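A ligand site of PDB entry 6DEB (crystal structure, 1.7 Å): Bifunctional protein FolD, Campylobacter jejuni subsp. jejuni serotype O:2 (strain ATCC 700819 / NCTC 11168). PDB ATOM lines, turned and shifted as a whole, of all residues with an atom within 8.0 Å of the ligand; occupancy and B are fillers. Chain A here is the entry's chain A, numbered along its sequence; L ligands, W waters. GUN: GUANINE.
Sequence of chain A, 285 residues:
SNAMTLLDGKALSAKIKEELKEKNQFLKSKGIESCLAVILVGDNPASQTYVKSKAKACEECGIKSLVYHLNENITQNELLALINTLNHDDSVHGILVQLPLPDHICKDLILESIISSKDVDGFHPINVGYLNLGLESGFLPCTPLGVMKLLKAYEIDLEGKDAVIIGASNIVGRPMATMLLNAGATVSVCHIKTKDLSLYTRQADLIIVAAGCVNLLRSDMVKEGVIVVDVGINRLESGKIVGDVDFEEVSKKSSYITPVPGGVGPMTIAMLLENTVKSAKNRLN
N of Gln 98 is in hydrogen-bond range of O of Ile 39, at 2.9 Å.
The side-chain hydroxyl of Thr 143 lies close to the side-chain hydroxyl of Thr 268, 3.3 Å away.
The side-chain amino group of Lys 54 sits at hydrogen-bond distance from the side-chain amide oxygen of Gln 98.
The backbone NH (N) of Ile 39 is in hydrogen-bond range of the backbone carbonyl oxygen (O) of Leu 96 (2.9 Å).
The backbone carbonyl oxygen of Leu 99 sits close to an oxygen (O6) of the ligand, at 3.2 Å.
Merely in contact with the ligand: Ile 171, Thr 143, Gln 98, Leu 96 and Phe 123.
Hydrophobic or aromatic side chains that line the ligand: Leu 96, Leu 99, Phe 123 and Ile 171.
Eight residues have an atom within 4 Å of the ligand: Leu 96, Val 97, Gln 98, Leu 99, Asp 121, Phe 123, Thr 143 and Ile 171.
The nearest printed residue that does not touch the ligand is Lys 54 (4.3 Å).
Water W1 lies within hydrogen-bond range of a nitrogen (N9) of the ligand (2.8 Å) and the side-chain carboxylate of Asp 121 (2.9 Å).
A nitrogen (N2) of the ligand sits at hydrogen-bond distance from the backbone carbonyl oxygen (O) of Val 97.
A nitrogen (N2) of the ligand lies within hydrogen-bond range of the side-chain carboxylate of Asp 121 (2.7 Å).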
ATOM      1  N   VAL A  38      17.911   6.603  18.424  1.00  0.00           N
ATOM      2  CA  VAL A  38      18.670   6.550  17.174  1.00  0.00           C
ATOM      3  C   VAL A  38      18.114   7.595  16.229  1.00  0.00           C
ATOM      4  O   VAL A  38      16.897   7.682  16.003  1.00  0.00           O
ATOM      5  CB  VAL A  38      18.559   5.140  16.515  1.00  0.00           C
ATOM      6  CG1 VAL A  38      19.333   5.106  15.197  1.00  0.00           C
ATOM      7  CG2 VAL A  38      19.094   4.060  17.471  1.00  0.00           C
ATOM      8  N   ILE A  39      18.994   8.430  15.692  1.00  0.00           N
ATOM      9  CA  ILE A  39      18.584   9.474  14.750  1.00  0.00           C
ATOM     10  C   ILE A  39      19.102   9.150  13.361  1.00  0.00           C
ATOM     11  O   ILE A  39      20.316   9.012  13.146  1.00  0.00           O
ATOM     12  CB  ILE A  39      19.085  10.853  15.178  1.00  0.00           C
ATOM     13  CG1 ILE A  39      18.589  11.176  16.605  1.00  0.00           C
ATOM     14  CG2 ILE A  39      18.639  11.902  14.135  1.00  0.00           C
ATOM     15  CD1 ILE A  39      19.302  12.371  17.227  1.00  0.00           C
ATOM     16  N   SER A  47      21.881   2.816   5.395  1.00  0.00           N
ATOM     17  CA  SER A  47      21.577   3.420   6.699  1.00  0.00           C
ATOM     18  C   SER A  47      20.254   2.921   7.282  1.00  0.00           C
ATOM     19  O   SER A  47      20.158   2.679   8.490  1.00  0.00           O
ATOM     20  CB  SER A  47      21.572   4.950   6.583  1.00  0.00           C
ATOM     21  OG  SER A  47      22.861   5.422   6.219  1.00  0.00           O
ATOM     22  N   TYR A  50      20.816  -0.590   8.558  1.00  0.00           N
ATOM     23  CA  TYR A  50      21.582  -0.553   9.801  1.00  0.00           C
ATOM     24  C   TYR A  50      20.715  -0.144  10.993  1.00  0.00           C
ATOM     25  O   TYR A  50      20.809  -0.729  12.064  1.00  0.00           O
ATOM     26  CB  TYR A  50      22.753   0.425   9.706  1.00  0.00           C
ATOM     27  CG  TYR A  50      23.853   0.015   8.757  1.00  0.00           C
ATOM     28  CD1 TYR A  50      24.327  -1.285   8.740  1.00  0.00           C
ATOM     29  CD2 TYR A  50      24.413   0.940   7.882  1.00  0.00           C
ATOM     30  CE1 TYR A  50      25.335  -1.667   7.861  1.00  0.00           C
ATOM     31  CE2 TYR A  50      25.414   0.570   7.001  1.00  0.00           C
ATOM     32  CZ  TYR A  50      25.877  -0.743   7.002  1.00  0.00           C
ATOM     33  OH  TYR A  50      26.881  -1.109   6.138  1.00  0.00           O
ATOM     34  N   LYS A  54      19.659  -2.206  14.460  1.00  0.00           N
ATOM     35  CA  LYS A  54      19.910  -1.732  15.816  1.00  0.00           C
ATOM     36  C   LYS A  54      18.612  -1.781  16.605  1.00  0.00           C
ATOM     37  O   LYS A  54      18.579  -2.220  17.754  1.00  0.00           O
ATOM     38  CB  LYS A  54      20.517  -0.329  15.787  1.00  0.00           C
ATOM     39  CG  LYS A  54      21.898  -0.303  15.159  1.00  0.00           C
ATOM     40  CD  LYS A  54      22.485   1.102  14.996  1.00  0.00           C
ATOM     41  CE  LYS A  54      23.756   0.996  14.159  1.00  0.00           C
ATOM     42  NZ  LYS A  54      24.458   2.271  13.893  1.00  0.00           N
ATOM     43  N   ILE A  95      22.272   8.179  22.950  1.00  0.00           N
ATOM     44  CA  ILE A  95      21.880   8.890  21.739  1.00  0.00           C
ATOM     45  C   ILE A  95      22.905   8.527  20.665  1.00  0.00           C
ATOM     46  O   ILE A  95      24.099   8.695  20.889  1.00  0.00           O
ATOM     47  CB  ILE A  95      21.920  10.423  21.968  1.00  0.00           C
ATOM     48  CG1 ILE A  95      20.885  10.843  23.015  1.00  0.00           C
ATOM     49  CG2 ILE A  95      21.696  11.193  20.648  1.00  0.00           C
ATOM     50  CD1 ILE A  95      21.174  12.249  23.629  1.00  0.00           C
ATOM     51  N   LEU A  96      22.427   8.012  19.543  1.00  0.00           N
ATOM     52  CA  LEU A  96      23.298   7.681  18.413  1.00  0.00           C
ATOM     53  C   LEU A  96      22.779   8.418  17.178  1.00  0.00           C
ATOM     54  O   LEU A  96      21.591   8.401  16.875  1.00  0.00           O
ATOM     55  CB  LEU A  96      23.245   6.172  18.152  1.00  0.00           C
ATOM     56  CG  LEU A  96      24.051   5.618  16.984  1.00  0.00           C
ATOM     57  CD1 LEU A  96      24.558   4.230  17.381  1.00  0.00           C
ATOM     58  CD2 LEU A  96      23.237   5.545  15.699  1.00  0.00           C
ATOM     59  N   VAL A  97      23.699   9.041  16.444  1.00  0.00           N
ATOM     60  CA  VAL A  97      23.371   9.585  15.132  1.00  0.00           C
ATOM     61  C   VAL A  97      23.951   8.713  14.042  1.00  0.00           C
ATOM     62  O   VAL A  97      25.172   8.523  13.944  1.00  0.00           O
ATOM     63  CB  VAL A  97      23.911  11.015  14.986  1.00  0.00           C
ATOM     64  CG1 VAL A  97      23.723  11.521  13.559  1.00  0.00           C
ATOM     65  CG2 VAL A  97      23.236  11.913  16.032  1.00  0.00           C
ATOM     66  N   GLN A  98      23.082   8.151  13.203  1.00  0.00           N
ATOM     67  CA  GLN A  98      23.534   7.260  12.158  1.00  0.00           C
ATOM     68  C   GLN A  98      24.326   8.040  11.120  1.00  0.00           C
ATOM     69  O   GLN A  98      23.876   9.071  10.606  1.00  0.00           O
ATOM     70  CB  GLN A  98      22.326   6.546  11.534  1.00  0.00           C
ATOM     71  CG  GLN A  98      22.679   5.543  10.466  1.00  0.00           C
ATOM     72  CD  GLN A  98      23.423   4.343  11.008  1.00  0.00           C
ATOM     73  OE1 GLN A  98      23.137   3.851  12.104  1.00  0.00           O
ATOM     74  NE2 GLN A  98      24.404   3.869  10.267  1.00  0.00           N
ATOM     75  N   LEU A  99      25.544   7.584  10.835  1.00  0.00           N
ATOM     76  CA  LEU A  99      26.381   8.262   9.832  1.00  0.00           C
ATOM     77  C   LEU A  99      26.313   7.480   8.526  1.00  0.00           C
ATOM     78  O   LEU A  99      26.167   6.263   8.535  1.00  0.00           O
ATOM     79  CB  LEU A  99      27.826   8.377  10.329  1.00  0.00           C
ATOM     80  CG  LEU A  99      27.993   9.064  11.680  1.00  0.00           C
ATOM     81  CD1 LEU A  99      29.447   8.998  12.168  1.00  0.00           C
ATOM     82  CD2 LEU A  99      27.490  10.505  11.627  1.00  0.00           C
ATOM     83  N   PRO A 100      26.434   8.185   7.382  1.00  0.00           N
ATOM     84  CA  PRO A 100      26.809   9.600   7.276  1.00  0.00           C
ATOM     85  C   PRO A 100      25.610  10.555   7.313  1.00  0.00           C
ATOM     86  O   PRO A 100      24.489  10.169   6.978  1.00  0.00           O
ATOM     87  CB  PRO A 100      27.465   9.649   5.890  1.00  0.00           C
ATOM     88  CG  PRO A 100      26.617   8.690   5.083  1.00  0.00           C
ATOM     89  CD  PRO A 100      26.197   7.583   6.054  1.00  0.00           C
ATOM     90  N   LEU A 111      28.198  15.653  16.491  1.00  0.00           N
ATOM     91  CA  LEU A 111      28.666  14.641  17.455  1.00  0.00           C
ATOM     92  C   LEU A 111      29.095  15.260  18.797  1.00  0.00           C
ATOM     93  O   LEU A 111      28.842  14.687  19.865  1.00  0.00           O
ATOM     94  CB  LEU A 111      29.807  13.821  16.843  1.00  0.00           C
ATOM     95  CG  LEU A 111      29.325  13.059  15.596  1.00  0.00           C
ATOM     96  CD1 LEU A 111      30.453  12.268  14.946  1.00  0.00           C
ATOM     97  CD2 LEU A 111      28.147  12.153  15.944  1.00  0.00           C
ATOM     98  N   ILE A 114      26.156  15.991  21.329  1.00  0.00           N
ATOM     99  CA  ILE A 114      25.563  14.931  22.149  1.00  0.00           C
ATOM    100  C   ILE A 114      26.188  14.983  23.541  1.00  0.00           C
ATOM    101  O   ILE A 114      27.399  15.142  23.642  1.00  0.00           O
ATOM    102  CB  ILE A 114      25.822  13.556  21.520  1.00  0.00           C
ATOM    103  CG1 ILE A 114      25.198  13.473  20.140  1.00  0.00           C
ATOM    104  CG2 ILE A 114      25.297  12.436  22.439  1.00  0.00           C
ATOM    105  CD1 ILE A 114      25.620  12.246  19.348  1.00  0.00           C
ATOM    106  N   VAL A 120      26.920   6.885  23.352  1.00  0.00           N
ATOM    107  CA  VAL A 120      27.160   5.446  23.294  1.00  0.00           C
ATOM    108  C   VAL A 120      28.060   5.007  22.125  1.00  0.00           C
ATOM    109  O   VAL A 120      28.610   3.912  22.141  1.00  0.00           O
ATOM    110  CB  VAL A 120      25.820   4.659  23.293  1.00  0.00           C
ATOM    111  CG1 VAL A 120      25.137   4.788  24.674  1.00  0.00           C
ATOM    112  CG2 VAL A 120      24.893   5.155  22.143  1.00  0.00           C
ATOM    113  N   ASP A 121      28.247   5.864  21.117  1.00  0.00           N
ATOM    114  CA  ASP A 121      29.199   5.582  20.050  1.00  0.00           C
ATOM    115  C   ASP A 121      30.630   5.981  20.445  1.00  0.00           C
ATOM    116  O   ASP A 121      31.597   5.633  19.773  1.00  0.00           O
ATOM    117  CB  ASP A 121      28.803   6.343  18.776  1.00  0.00           C
ATOM    118  CG  ASP A 121      28.121   5.464  17.741  1.00  0.00           C
ATOM    119  OD1 ASP A 121      28.495   4.282  17.561  1.00  0.00           O
ATOM    120  OD2 ASP A 121      27.192   5.982  17.088  1.00  0.00           O
ATOM    121  N   GLY A 122      30.798   6.706  21.553  1.00  0.00           N
ATOM    122  CA  GLY A 122      32.136   7.094  21.954  1.00  0.00           C
ATOM    123  C   GLY A 122      32.824   8.099  21.010  1.00  0.00           C
ATOM    124  O   GLY A 122      34.048   8.215  20.983  1.00  0.00           O
ATOM    125  N   PHE A 123      32.019   8.870  20.259  1.00  0.00           N
ATOM    126  CA  PHE A 123      32.567   9.821  19.285  1.00  0.00           C
ATOM    127  C   PHE A 123      32.833  11.234  19.825  1.00  0.00           C
ATOM    128  O   PHE A 123      33.559  12.000  19.190  1.00  0.00           O
ATOM    129  CB  PHE A 123      31.622   9.964  18.076  1.00  0.00           C
ATOM    130  CG  PHE A 123      31.505   8.707  17.243  1.00  0.00           C
ATOM    131  CD1 PHE A 123      32.488   7.729  17.289  1.00  0.00           C
ATOM    132  CD2 PHE A 123      30.393   8.507  16.429  1.00  0.00           C
ATOM    133  CE1 PHE A 123      32.366   6.546  16.515  1.00  0.00           C
ATOM    134  CE2 PHE A 123      30.273   7.334  15.664  1.00  0.00           C
ATOM    135  CZ  PHE A 123      31.251   6.362  15.716  1.00  0.00           C
ATOM    136  N   PRO A 141      34.336   3.478  21.467  1.00  0.00           N
ATOM    137  CA  PRO A 141      33.606   3.211  20.220  1.00  0.00           C
ATOM    138  C   PRO A 141      33.306   1.732  20.014  1.00  0.00           C
ATOM    139  O   PRO A 141      34.123   0.873  20.369  1.00  0.00           O
ATOM    140  CB  PRO A 141      34.558   3.718  19.116  1.00  0.00           C
ATOM    141  CG  PRO A 141      35.422   4.745  19.845  1.00  0.00           C
ATOM    142  CD  PRO A 141      35.624   4.145  21.221  1.00  0.00           C
ATOM    143  N   CYS A 142      32.151   1.455  19.454  1.00  0.00           N
ATOM    144  CA  CYS A 142      31.595   0.121  19.470  1.00  0.00           C
ATOM    145  C   CYS A 142      32.350  -0.881  18.620  1.00  0.00           C
ATOM    146  O   CYS A 142      32.475  -2.042  19.003  1.00  0.00           O
ATOM    147  CB  CYS A 142      30.126   0.134  19.031  1.00  0.00           C
ATOM    148  SG  CYS A 142      29.066   1.148  20.110  1.00  0.00           S
ATOM    149  N   THR A 143      32.842  -0.468  17.457  1.00  0.00           N
ATOM    150  CA  THR A 143      33.534  -1.453  16.618  1.00  0.00           C
ATOM    151  C   THR A 143      34.862  -1.935  17.229  1.00  0.00           C
ATOM    152  O   THR A 143      35.032  -3.152  17.396  1.00  0.00           O
ATOM    153  CB  THR A 143      33.741  -0.919  15.169  1.00  0.00           C
ATOM    154  OG1 THR A 143      32.463  -0.617  14.600  1.00  0.00           O
ATOM    155  CG2 THR A 143      34.427  -1.966  14.313  1.00  0.00           C
ATOM    156  N   PRO A 144      35.769  -1.016  17.609  1.00  0.00           N
ATOM    157  CA  PRO A 144      37.004  -1.521  18.240  1.00  0.00           C
ATOM    158  C   PRO A 144      36.737  -2.187  19.571  1.00  0.00           C
ATOM    159  O   PRO A 144      37.411  -3.159  19.896  1.00  0.00           O
ATOM    160  CB  PRO A 144      37.875  -0.282  18.431  1.00  0.00           C
ATOM    161  CG  PRO A 144      36.918   0.911  18.252  1.00  0.00           C
ATOM    162  CD  PRO A 144      35.838   0.439  17.352  1.00  0.00           C
ATOM    163  N   ILE A 171      36.072   6.242  13.363  1.00  0.00           N
ATOM    164  CA  ILE A 171      35.092   5.240  13.782  1.00  0.00           C
ATOM    165  C   ILE A 171      35.710   3.912  14.178  1.00  0.00           C
ATOM    166  O   ILE A 171      35.242   3.260  15.106  1.00  0.00           O
ATOM    167  CB  ILE A 171      34.018   5.030  12.672  1.00  0.00           C
ATOM    168  CG1 ILE A 171      33.267   6.328  12.409  1.00  0.00           C
ATOM    169  CG2 ILE A 171      33.031   3.892  13.060  1.00  0.00           C
ATOM    170  CD1 ILE A 171      32.218   6.206  11.324  1.00  0.00           C
ATOM    171  N   VAL A 172      36.778   3.513  13.482  1.00  0.00           N
ATOM    172  CA  VAL A 172      37.430   2.234  13.752  1.00  0.00           C
ATOM    173  C   VAL A 172      38.931   2.311  13.979  1.00  0.00           C
ATOM    174  O   VAL A 172      39.416   1.979  15.051  1.00  0.00           O
ATOM    175  CB  VAL A 172      37.193   1.217  12.597  1.00  0.00           C
ATOM    176  CG1 VAL A 172      37.814  -0.126  12.978  1.00  0.00           C
ATOM    177  CG2 VAL A 172      35.712   1.059  12.316  1.00  0.00           C
ATOM    178  N   VAL A 231      37.128  -6.140   9.498  1.00  0.00           N
ATOM    179  CA  VAL A 231      36.037  -5.216   9.740  1.00  0.00           C
ATOM    180  C   VAL A 231      35.248  -4.871   8.462  1.00  0.00           C
ATOM    181  O   VAL A 231      34.192  -4.257   8.511  1.00  0.00           O
ATOM    182  CB  VAL A 231      36.579  -3.908  10.414  1.00  0.00           C
ATOM    183  CG1 VAL A 231      35.451  -2.974  10.824  1.00  0.00           C
ATOM    184  CG2 VAL A 231      37.387  -4.249  11.608  1.00  0.00           C
ATOM    185  N   THR A 268      29.738  -5.321  16.941  1.00  0.00           N
ATOM    186  CA  THR A 268      29.606  -3.875  16.960  1.00  0.00           C
ATOM    187  C   THR A 268      28.248  -3.514  17.525  1.00  0.00           C
ATOM    188  O   THR A 268      28.124  -2.613  18.374  1.00  0.00           O
ATOM    189  CB  THR A 268      29.783  -3.280  15.561  1.00  0.00           C
ATOM    190  OG1 THR A 268      31.106  -3.579  15.089  1.00  0.00           O
ATOM    191  CG2 THR A 268      29.590  -1.756  15.651  1.00  0.00           C
ATOM    192  N   ILE A 269      27.237  -4.228  17.080  1.00  0.00           N
ATOM    193  CA  ILE A 269      25.884  -3.997  17.602  1.00  0.00           C
ATOM    194  C   ILE A 269      25.800  -4.382  19.078  1.00  0.00           C
ATOM    195  O   ILE A 269      25.215  -3.663  19.880  1.00  0.00           O
ATOM    196  CB  ILE A 269      24.845  -4.778  16.803  1.00  0.00           C
ATOM    197  CG1 ILE A 269      24.732  -4.214  15.378  1.00  0.00           C
ATOM    198  CG2 ILE A 269      23.499  -4.729  17.541  1.00  0.00           C
ATOM    199  CD1 ILE A 269      23.977  -5.126  14.421  1.00  0.00           C
ATOM    200  N   LEU A 272      27.043  -1.596  21.223  1.00  0.00           N
ATOM    201  CA  LEU A 272      26.105  -0.473  21.283  1.00  0.00           C
ATOM    202  C   LEU A 272      25.089  -0.723  22.392  1.00  0.00           C
ATOM    203  O   LEU A 272      24.758   0.174  23.186  1.00  0.00           O
ATOM    204  CB  LEU A 272      25.386  -0.337  19.947  1.00  0.00           C
ATOM    205  CG  LEU A 272      24.202   0.640  19.946  1.00  0.00           C
ATOM    206  CD1 LEU A 272      24.685   2.022  20.322  1.00  0.00           C
ATOM    207  CD2 LEU A 272      23.585   0.641  18.547  1.00  0.00           C
HETATM  208  N9  GUN L   1      29.605   2.400  14.262  1.00  0.00           N
HETATM  209  C8  GUN L   1      30.095   1.783  13.154  1.00  0.00           C
HETATM  210  N7  GUN L   1      29.653   2.383  12.013  1.00  0.00           N
HETATM  211  C5  GUN L   1      28.862   3.424  12.375  1.00  0.00           C
HETATM  212  C6  GUN L   1      28.083   4.480  11.672  1.00  0.00           C
HETATM  213  O6  GUN L   1      28.055   4.530  10.408  1.00  0.00           O
HETATM  214  N1  GUN L   1      27.400   5.367  12.414  1.00  0.00           N
HETATM  215  C2  GUN L   1      27.419   5.335  13.766  1.00  0.00           C
HETATM  216  N2  GUN L   1      26.712   6.254  14.459  1.00  0.00           N
HETATM  217  N3  GUN L   1      28.109   4.393  14.467  1.00  0.00           N
HETATM  218  C4  GUN L   1      28.845   3.431  13.855  1.00  0.00           C
HETATM  219  O   HOH W   1      27.968   1.734  16.371  1.00  0.00           O
HETATM  220  O   HOH W   2      26.350   1.232  11.524  1.00  0.00           O
